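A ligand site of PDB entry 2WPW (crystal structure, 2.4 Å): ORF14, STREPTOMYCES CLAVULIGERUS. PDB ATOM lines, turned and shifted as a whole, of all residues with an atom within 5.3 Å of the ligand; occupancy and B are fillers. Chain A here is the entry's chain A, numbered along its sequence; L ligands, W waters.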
ATOM      1  N   VAL A  87      39.196  12.448   8.772  1.00  0.00           N
ATOM      2  CA  VAL A  87      37.754  12.480   8.653  1.00  0.00           C
ATOM      3  C   VAL A  87      37.211  11.057   8.776  1.00  0.00           C
ATOM      4  O   VAL A  87      37.290  10.283   7.808  1.00  0.00           O
ATOM      5  CB  VAL A  87      37.346  13.050   7.267  1.00  0.00           C
ATOM      6  CG1 VAL A  87      35.819  12.878   7.046  1.00  0.00           C
ATOM      7  CG2 VAL A  87      37.758  14.535   7.101  1.00  0.00           C
ATOM      8  N   LEU A  90      31.673  11.371   7.172  1.00  0.00           N
ATOM      9  CA  LEU A  90      31.025  12.513   6.589  1.00  0.00           C
ATOM     10  C   LEU A  90      29.870  11.965   5.760  1.00  0.00           C
ATOM     11  O   LEU A  90      30.072  11.529   4.625  1.00  0.00           O
ATOM     12  CB  LEU A  90      32.012  13.324   5.762  1.00  0.00           C
ATOM     13  CG  LEU A  90      31.576  14.747   5.408  1.00  0.00           C
ATOM     14  CD1 LEU A  90      32.835  15.547   5.041  1.00  0.00           C
ATOM     15  CD2 LEU A  90      30.529  14.644   4.290  1.00  0.00           C
ATOM     16  N   LEU A  91      28.673  11.971   6.350  1.00  0.00           N
ATOM     17  CA  LEU A  91      27.550  11.178   5.868  1.00  0.00           C
ATOM     18  C   LEU A  91      26.254  11.986   5.788  1.00  0.00           C
ATOM     19  O   LEU A  91      25.879  12.663   6.730  1.00  0.00           O
ATOM     20  CB  LEU A  91      27.343  10.025   6.839  1.00  0.00           C
ATOM     21  CG  LEU A  91      26.174   9.090   6.573  1.00  0.00           C
ATOM     22  CD1 LEU A  91      26.163   8.632   5.161  1.00  0.00           C
ATOM     23  CD2 LEU A  91      26.169   7.844   7.568  1.00  0.00           C
ATOM     24  N   VAL A  92      25.559  11.940   4.653  1.00  0.00           N
ATOM     25  CA  VAL A  92      24.307  12.684   4.454  1.00  0.00           C
ATOM     26  C   VAL A  92      23.133  11.697   4.267  1.00  0.00           C
ATOM     27  O   VAL A  92      23.309  10.680   3.590  1.00  0.00           O
ATOM     28  CB  VAL A  92      24.458  13.603   3.265  1.00  0.00           C
ATOM     29  CG1 VAL A  92      23.160  14.312   2.894  1.00  0.00           C
ATOM     30  CG2 VAL A  92      25.593  14.612   3.529  1.00  0.00           C
ATOM     31  N   ARG A  96      18.354  13.101   1.233  1.00  0.00           N
ATOM     32  CA  ARG A  96      18.503  14.549   1.283  1.00  0.00           C
ATOM     33  C   ARG A  96      19.832  14.976   0.652  1.00  0.00           C
ATOM     34  O   ARG A  96      20.369  16.027   0.962  1.00  0.00           O
ATOM     35  CB  ARG A  96      18.357  15.080   2.718  1.00  0.00           C
ATOM     36  CG  ARG A  96      17.184  14.490   3.516  1.00  0.00           C
ATOM     37  CD  ARG A  96      15.951  15.379   3.548  1.00  0.00           C
ATOM     38  NE  ARG A  96      15.113  15.009   4.696  1.00  0.00           N
ATOM     39  CZ  ARG A  96      14.252  13.985   4.739  1.00  0.00           C
ATOM     40  NH1 ARG A  96      13.577  13.732   5.857  1.00  0.00           N
ATOM     41  NH2 ARG A  96      14.059  13.185   3.685  1.00  0.00           N
ATOM     42  N   ARG A  97      20.354  14.156  -0.257  1.00  0.00           N
ATOM     43  CA  ARG A  97      21.633  14.414  -0.878  1.00  0.00           C
ATOM     44  C   ARG A  97      21.493  15.477  -1.955  1.00  0.00           C
ATOM     45  O   ARG A  97      20.372  15.789  -2.416  1.00  0.00           O
ATOM     46  CB  ARG A  97      22.210  13.128  -1.498  1.00  0.00           C
ATOM     47  CG  ARG A  97      21.979  11.886  -0.657  1.00  0.00           C
ATOM     48  CD  ARG A  97      23.216  11.418   0.100  1.00  0.00           C
ATOM     49  NE  ARG A  97      23.672  10.146  -0.450  1.00  0.00           N
ATOM     50  CZ  ARG A  97      23.959   9.017   0.213  1.00  0.00           C
ATOM     51  NH1 ARG A  97      23.918   8.909   1.527  1.00  0.00           N
ATOM     52  NH2 ARG A  97      24.341   7.974  -0.519  1.00  0.00           N
ATOM     53  N   ARG A  98      22.610  16.061  -2.365  1.00  0.00           N
ATOM     54  CA  ARG A  98      22.583  16.967  -3.484  1.00  0.00           C
ATOM     55  C   ARG A  98      21.794  18.243  -3.133  1.00  0.00           C
ATOM     56  O   ARG A  98      21.148  18.846  -4.011  1.00  0.00           O
ATOM     57  CB  ARG A  98      21.934  16.257  -4.690  1.00  0.00           C
ATOM     58  CG  ARG A  98      22.754  15.084  -5.231  1.00  0.00           C
ATOM     59  CD  ARG A  98      24.161  15.546  -5.462  1.00  0.00           C
ATOM     60  NE  ARG A  98      24.662  14.962  -6.677  1.00  0.00           N
ATOM     61  CZ  ARG A  98      25.191  15.632  -7.676  1.00  0.00           C
ATOM     62  NH1 ARG A  98      25.355  16.954  -7.592  1.00  0.00           N
ATOM     63  NH2 ARG A  98      25.582  14.935  -8.723  1.00  0.00           N
ATOM     64  N   ARG A  99      21.815  18.652  -1.858  1.00  0.00           N
ATOM     65  CA  ARG A  99      21.211  19.925  -1.501  1.00  0.00           C
ATOM     66  C   ARG A  99      22.232  20.844  -0.864  1.00  0.00           C
ATOM     67  O   ARG A  99      21.878  21.956  -0.506  1.00  0.00           O
ATOM     68  CB  ARG A  99      20.070  19.739  -0.522  1.00  0.00           C
ATOM     69  CG  ARG A  99      19.009  18.822  -1.008  1.00  0.00           C
ATOM     70  CD  ARG A  99      18.030  18.589   0.102  1.00  0.00           C
ATOM     71  NE  ARG A  99      16.879  17.795  -0.322  1.00  0.00           N
ATOM     72  CZ  ARG A  99      15.757  17.709   0.369  1.00  0.00           C
ATOM     73  NH1 ARG A  99      15.616  18.356   1.519  1.00  0.00           N
ATOM     74  NH2 ARG A  99      14.762  16.962  -0.094  1.00  0.00           N
ATOM     75  N   GLY A 100      23.478  20.383  -0.669  1.00  0.00           N
ATOM     76  CA  GLY A 100      24.493  21.237  -0.063  1.00  0.00           C
ATOM     77  C   GLY A 100      24.903  20.818   1.352  1.00  0.00           C
ATOM     78  O   GLY A 100      25.749  21.445   2.003  1.00  0.00           O
ATOM     79  N   ILE A 101      24.307  19.759   1.853  1.00  0.00           N
ATOM     80  CA  ILE A 101      24.597  19.390   3.213  1.00  0.00           C
ATOM     81  C   ILE A 101      26.044  18.954   3.315  1.00  0.00           C
ATOM     82  O   ILE A 101      26.787  19.471   4.159  1.00  0.00           O
ATOM     83  CB  ILE A 101      23.598  18.289   3.732  1.00  0.00           C
ATOM     84  CG1 ILE A 101      22.142  18.812   3.693  1.00  0.00           C
ATOM     85  CG2 ILE A 101      24.016  17.857   5.097  1.00  0.00           C
ATOM     86  CD1 ILE A 101      20.995  17.756   3.975  1.00  0.00           C
ATOM     87  N   GLY A 102      26.452  18.026   2.479  1.00  0.00           N
ATOM     88  CA  GLY A 102      27.810  17.549   2.492  1.00  0.00           C
ATOM     89  C   GLY A 102      28.778  18.699   2.404  1.00  0.00           C
ATOM     90  O   GLY A 102      29.790  18.787   3.147  1.00  0.00           O
ATOM     91  N   ARG A 103      28.482  19.620   1.513  1.00  0.00           N
ATOM     92  CA  ARG A 103      29.345  20.787   1.367  1.00  0.00           C
ATOM     93  C   ARG A 103      29.468  21.514   2.718  1.00  0.00           C
ATOM     94  O   ARG A 103      30.546  21.979   3.088  1.00  0.00           O
ATOM     95  CB  ARG A 103      28.799  21.743   0.264  1.00  0.00           C
ATOM     96  CG  ARG A 103      29.797  22.823  -0.182  1.00  0.00           C
ATOM     97  CD  ARG A 103      29.140  23.830  -1.118  1.00  0.00           C
ATOM     98  NE  ARG A 103      28.935  23.300  -2.470  1.00  0.00           N
ATOM     99  CZ  ARG A 103      29.903  23.207  -3.376  1.00  0.00           C
ATOM    100  NH1 ARG A 103      31.131  23.626  -3.083  1.00  0.00           N
ATOM    101  NH2 ARG A 103      29.657  22.713  -4.579  1.00  0.00           N
ATOM    102  N   ALA A 104      28.361  21.557   3.456  1.00  0.00           N
ATOM    103  CA  ALA A 104      28.307  22.371   4.657  1.00  0.00           C
ATOM    104  C   ALA A 104      29.079  21.622   5.760  1.00  0.00           C
ATOM    105  O   ALA A 104      29.788  22.222   6.522  1.00  0.00           O
ATOM    106  CB  ALA A 104      26.868  22.633   5.071  1.00  0.00           C
ATOM    107  N   TRP A 106      31.547  19.724   5.150  1.00  0.00           N
ATOM    108  CA  TRP A 106      32.975  19.787   4.826  1.00  0.00           C
ATOM    109  C   TRP A 106      33.581  21.137   5.195  1.00  0.00           C
ATOM    110  O   TRP A 106      34.740  21.207   5.583  1.00  0.00           O
ATOM    111  CB  TRP A 106      33.220  19.468   3.357  1.00  0.00           C
ATOM    112  CG  TRP A 106      34.595  19.711   2.922  1.00  0.00           C
ATOM    113  CD1 TRP A 106      35.087  20.855   2.298  1.00  0.00           C
ATOM    114  CD2 TRP A 106      35.686  18.812   3.014  1.00  0.00           C
ATOM    115  NE1 TRP A 106      36.393  20.687   2.002  1.00  0.00           N
ATOM    116  CE2 TRP A 106      36.794  19.449   2.418  1.00  0.00           C
ATOM    117  CE3 TRP A 106      35.836  17.529   3.525  1.00  0.00           C
ATOM    118  CZ2 TRP A 106      38.037  18.861   2.364  1.00  0.00           C
ATOM    119  CZ3 TRP A 106      37.051  16.927   3.420  1.00  0.00           C
ATOM    120  CH2 TRP A 106      38.139  17.593   2.862  1.00  0.00           C
ATOM    121  N   ALA A 123      41.094  11.439   4.418  1.00  0.00           N
ATOM    122  CA  ALA A 123      39.920  10.595   4.392  1.00  0.00           C
ATOM    123  C   ALA A 123      40.195   9.343   3.611  1.00  0.00           C
ATOM    124  O   ALA A 123      41.097   9.272   2.790  1.00  0.00           O
ATOM    125  CB  ALA A 123      38.760  11.358   3.778  1.00  0.00           C
ATOM    126  N   VAL A 125      38.276   6.852   0.927  1.00  0.00           N
ATOM    127  CA  VAL A 125      37.147   7.027   0.011  1.00  0.00           C
ATOM    128  C   VAL A 125      36.979   5.748  -0.755  1.00  0.00           C
ATOM    129  O   VAL A 125      37.961   5.258  -1.325  1.00  0.00           O
ATOM    130  CB  VAL A 125      37.408   8.198  -0.975  1.00  0.00           C
ATOM    131  CG1 VAL A 125      36.279   8.352  -2.029  1.00  0.00           C
ATOM    132  CG2 VAL A 125      37.640   9.509  -0.206  1.00  0.00           C
ATOM    133  N   ASP A 136      29.974   3.080  -6.668  1.00  0.00           N
ATOM    134  CA  ASP A 136      29.421   4.404  -6.766  1.00  0.00           C
ATOM    135  C   ASP A 136      30.580   5.423  -6.928  1.00  0.00           C
ATOM    136  O   ASP A 136      31.465   5.507  -6.086  1.00  0.00           O
ATOM    137  CB  ASP A 136      28.570   4.717  -5.531  1.00  0.00           C
ATOM    138  CG  ASP A 136      27.634   5.922  -5.760  1.00  0.00           C
ATOM    139  OD1 ASP A 136      26.557   5.946  -5.131  1.00  0.00           O
ATOM    140  OD2 ASP A 136      27.972   6.841  -6.555  1.00  0.00           O
ATOM    141  N   GLY A 138      30.055   8.651  -6.726  1.00  0.00           N
ATOM    142  CA  GLY A 138      29.694   9.896  -6.049  1.00  0.00           C
ATOM    143  C   GLY A 138      30.739  10.367  -5.015  1.00  0.00           C
ATOM    144  O   GLY A 138      31.162  11.532  -5.029  1.00  0.00           O
ATOM    145  N   PRO A 139      31.125   9.486  -4.086  1.00  0.00           N
ATOM    146  CA  PRO A 139      31.979  10.018  -3.015  1.00  0.00           C
ATOM    147  C   PRO A 139      33.291  10.580  -3.549  1.00  0.00           C
ATOM    148  O   PRO A 139      33.768  11.569  -3.013  1.00  0.00           O
ATOM    149  CB  PRO A 139      32.224   8.818  -2.114  1.00  0.00           C
ATOM    150  CG  PRO A 139      31.524   7.679  -2.686  1.00  0.00           C
ATOM    151  CD  PRO A 139      30.573   8.177  -3.732  1.00  0.00           C
ATOM    152  N   ALA A 141      33.639  12.027  -6.548  1.00  0.00           N
ATOM    153  CA  ALA A 141      33.379  13.278  -7.197  1.00  0.00           C
ATOM    154  C   ALA A 141      33.140  14.376  -6.121  1.00  0.00           C
ATOM    155  O   ALA A 141      33.656  15.468  -6.263  1.00  0.00           O
ATOM    156  CB  ALA A 141      32.268  13.146  -8.179  1.00  0.00           C
ATOM    157  N   PHE A 142      32.412  14.056  -5.046  1.00  0.00           N
ATOM    158  CA  PHE A 142      32.309  14.955  -3.822  1.00  0.00           C
ATOM    159  C   PHE A 142      33.685  15.426  -3.299  1.00  0.00           C
ATOM    160  O   PHE A 142      33.929  16.599  -3.105  1.00  0.00           O
ATOM    161  CB  PHE A 142      31.520  14.270  -2.680  1.00  0.00           C
ATOM    162  CG  PHE A 142      31.426  15.118  -1.431  1.00  0.00           C
ATOM    163  CD1 PHE A 142      30.607  16.235  -1.379  1.00  0.00           C
ATOM    164  CD2 PHE A 142      32.201  14.832  -0.323  1.00  0.00           C
ATOM    165  CE1 PHE A 142      30.551  17.025  -0.244  1.00  0.00           C
ATOM    166  CE2 PHE A 142      32.185  15.641   0.800  1.00  0.00           C
ATOM    167  CZ  PHE A 142      31.350  16.734   0.841  1.00  0.00           C
ATOM    168  N   ALA A 143      34.600  14.485  -3.159  1.00  0.00           N
ATOM    169  CA  ALA A 143      35.872  14.762  -2.590  1.00  0.00           C
ATOM    170  C   ALA A 143      36.603  15.756  -3.464  1.00  0.00           C
ATOM    171  O   ALA A 143      37.206  16.727  -2.953  1.00  0.00           O
ATOM    172  CB  ALA A 143      36.662  13.467  -2.480  1.00  0.00           C
ATOM    173  N   ALA A 145      35.305  17.731  -5.529  1.00  0.00           N
ATOM    174  CA  ALA A 145      34.573  18.949  -5.571  1.00  0.00           C
ATOM    175  C   ALA A 145      34.859  19.747  -4.309  1.00  0.00           C
ATOM    176  O   ALA A 145      34.838  20.960  -4.332  1.00  0.00           O
ATOM    177  CB  ALA A 145      33.107  18.666  -5.724  1.00  0.00           C
HETATM  178  N1  LIG L   1      27.785  12.645  -7.835  1.00  0.00           N
HETATM  179  C1  LIG L   1      28.485  13.603  -8.425  1.00  0.00           C
HETATM  180  N2  LIG L   1      28.828  14.703  -7.772  1.00  0.00           N
HETATM  181  C2  LIG L   1      28.538  14.877  -6.490  1.00  0.00           C
HETATM  182  C3  LIG L   1      27.822  13.897  -5.823  1.00  0.00           C
HETATM  183  C4  LIG L   1      27.446  12.736  -6.558  1.00  0.00           C
HETATM  184  N3  LIG L   1      26.769  11.695  -6.056  1.00  0.00           N
HETATM  185  N4  LIG L   1      27.672  14.309  -4.557  1.00  0.00           N
HETATM  186  C5  LIG L   1      28.263  15.497  -4.431  1.00  0.00           C
HETATM  187  N5  LIG L   1      28.792  15.839  -5.618  1.00  0.00           N
HETATM  188  C6  LIG L   1      29.573  17.074  -5.867  1.00  0.00           C
HETATM  189  C7  LIG L   1      28.853  17.920  -6.869  1.00  0.00           C
HETATM  190  O1  LIG L   1      29.814  18.764  -7.491  1.00  0.00           O
HETATM  191  C8  LIG L   1      27.991  18.781  -5.992  1.00  0.00           C
HETATM  192  O2  LIG L   1      27.952  20.079  -6.576  1.00  0.00           O
HETATM  193  P1  LIG L   1      26.492  20.842  -6.538  1.00  0.00           P
HETATM  194  O3  LIG L   1      26.345  22.239  -7.370  1.00  0.00           O
HETATM  195  O4  LIG L   1      25.210  19.914  -6.439  1.00  0.00           O
HETATM  196  O5  LIG L   1      26.464  20.165  -7.857  1.00  0.00           O
HETATM  197  C9  LIG L   1      28.664  18.808  -4.614  1.00  0.00           C
HETATM  198  O6  LIG L   1      29.782  17.913  -4.691  1.00  0.00           O
HETATM  199  C10 LIG L   1      27.716  17.980  -3.835  1.00  0.00           C
HETATM  200  O7  LIG L   1      27.517  18.578  -2.663  1.00  0.00           O
HETATM  201  P2  LIG L   1      26.331  18.140  -1.782  1.00  0.00           P
HETATM  202  O8  LIG L   1      26.758  18.722  -0.386  1.00  0.00           O
HETATM  203  O9  LIG L   1      24.929  18.550  -2.128  1.00  0.00           O
HETATM  204  O10 LIG L   1      26.251  16.576  -1.733  1.00  0.00           O
HETATM  205  P3  LIG L   1      25.587  15.596  -0.606  1.00  0.00           P
HETATM  206  O11 LIG L   1      24.543  14.717  -1.483  1.00  0.00           O
HETATM  207  O12 LIG L   1      25.168  16.248   0.631  1.00  0.00           O
HETATM  208  O13 LIG L   1      26.933  14.613  -0.424  1.00  0.00           O
HETATM  209  C11 LIG L   1      28.085  12.532   0.249  1.00  0.00           C
HETATM  210  C12 LIG L   1      27.148  13.760   0.613  1.00  0.00           C
HETATM  211  C13 LIG L   1      28.382  13.213  -1.060  1.00  0.00           C
HETATM  212  C14 LIG L   1      28.806  12.942   1.564  1.00  0.00           C
HETATM  213  C15 LIG L   1      26.842  11.564   0.271  1.00  0.00           C
HETATM  214  O14 LIG L   1      26.823  10.976  -1.003  1.00  0.00           O
HETATM  215  C16 LIG L   1      27.039  10.521   1.370  1.00  0.00           C
HETATM  216  O15 LIG L   1      26.783  10.777   2.573  1.00  0.00           O
HETATM  217  N6  LIG L   1      27.560   9.364   0.917  1.00  0.00           N
HETATM  218  C17 LIG L   1      27.862   8.223   1.767  1.00  0.00           C
HETATM  219  C18 LIG L   1      28.981   8.570   2.756  1.00  0.00           C
HETATM  220  C19 LIG L   1      30.277   8.948   2.051  1.00  0.00           C
HETATM  221  O16 LIG L   1      30.639   8.315   1.069  1.00  0.00           O
HETATM  222  N7  LIG L   1      31.002   9.931   2.609  1.00  0.00           N
HETATM  223  C20 LIG L   1      32.386  10.285   2.198  1.00  0.00           C
HETATM  224  C21 LIG L   1      32.488  11.349   1.097  1.00  0.00           C
HETATM  225  S1  LIG L   1      34.253  11.657   0.678  1.00  0.00           S
HETATM  226  C22 LIG L   1      34.804  12.752   1.964  1.00  0.00           C
HETATM  227  O17 LIG L   1      34.045  13.121   2.872  1.00  0.00           O
HETATM  228  C23 LIG L   1      36.207  13.288   1.922  1.00  0.00           C
HETATM  229  O   HOH W   1      26.298   8.938  -7.147  1.00  0.00           O
HETATM  230  O   HOH W   2      33.436   6.417   0.560  1.00  0.00           O
HETATM  231  O   HOH W   3      22.505  17.746   0.513  1.00  0.00           O
HETATM  232  O   HOH W   4      23.617  12.540  -7.265  1.00  0.00           O
HETATM  233  O   HOH W   5      27.515   4.890   2.469  1.00  0.00           O
HETATM  234  O   HOH W   6      31.161  16.065  -9.227  1.00  0.00           O
HETATM  235  O   HOH W   7      24.448  23.847  -8.457  1.00  0.00           O
HETATM  236  O   HOH W   8      30.971  21.629  -7.258  1.00  0.00           O
HETATM  237  O   HOH W   9      27.277   9.433  -3.438  1.00  0.00           O
HETATM  238  O   HOH W  10      31.427   8.567   5.768  1.00  0.00           O
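N of Arg 98 sits at hydrogen-bond distance from O11 of the ligand (2.5 Å). An oxygen (O4) of the ligand is in salt-bridge range of the guanidinium group of Arg 98 (3.2 Å). An oxygen (O15) of the ligand lies within hydrogen-bond range of the backbone NH (N) of Val 92, 2.7 Å away. N of Arg 103 is in hydrogen-bond range of O8 of the ligand (2.7 Å). O of Leu 90 is in hydrogen-bond range of N7 of the ligand (2.7 Å). An oxygen (O9) of the ligand is in hydrogen-bond range of the backbone NH (N) of Gly 100. The guanidinium group (NE) of Arg 97 sits at hydrogen-bond distance from an oxygen (O14) of the ligand. The backbone NH (N) of Gly 102 is in hydrogen-bond range of an oxygen (O12) of the ligand (2.9 Å). N of Arg 99 lies within hydrogen-bond range of O9 of the ligand, 3.1 Å away. N of Ile 101 is in hydrogen-bond range of O8 of the ligand, 3.5 Å away.
The backbone carbonyl oxygen (O) of Val 92 lies within hydrogen-bond range of the guanidinium group (NH1) of Arg 97 (2.8 Å). The backbone NH (N) of Gly 138 sits at hydrogen-bond distance from the side-chain carboxylate (OD2) of Asp 136 (2.8 Å).
O of Pro 139 sits close to S1 of the ligand (3.7 Å). Merely in contact with the ligand: Leu 91, Gly 138, Ala 145, Phe 142, Ala 123 and Ala 141. The nearest printed residue that does not touch the ligand is Trp 106 (4.02 Å).
Water W1 bridges OD2 of Asp 136 (2.7 Å) and N3 of the ligand (3.0 Å). Water W8 lies within hydrogen-bond range of an oxygen (O1) of the ligand (3.1 Å) and the guanidinium group of Arg 103 (3.2 Å). Water W10 lies within hydrogen-bond range of the backbone NH of Leu 90 and a nitrogen (N7) of the ligand. Water W4 bridges the guanidinium group of Arg 98 (2.7 Å) and a nitrogen (N3) of the ligand (3.5 Å).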
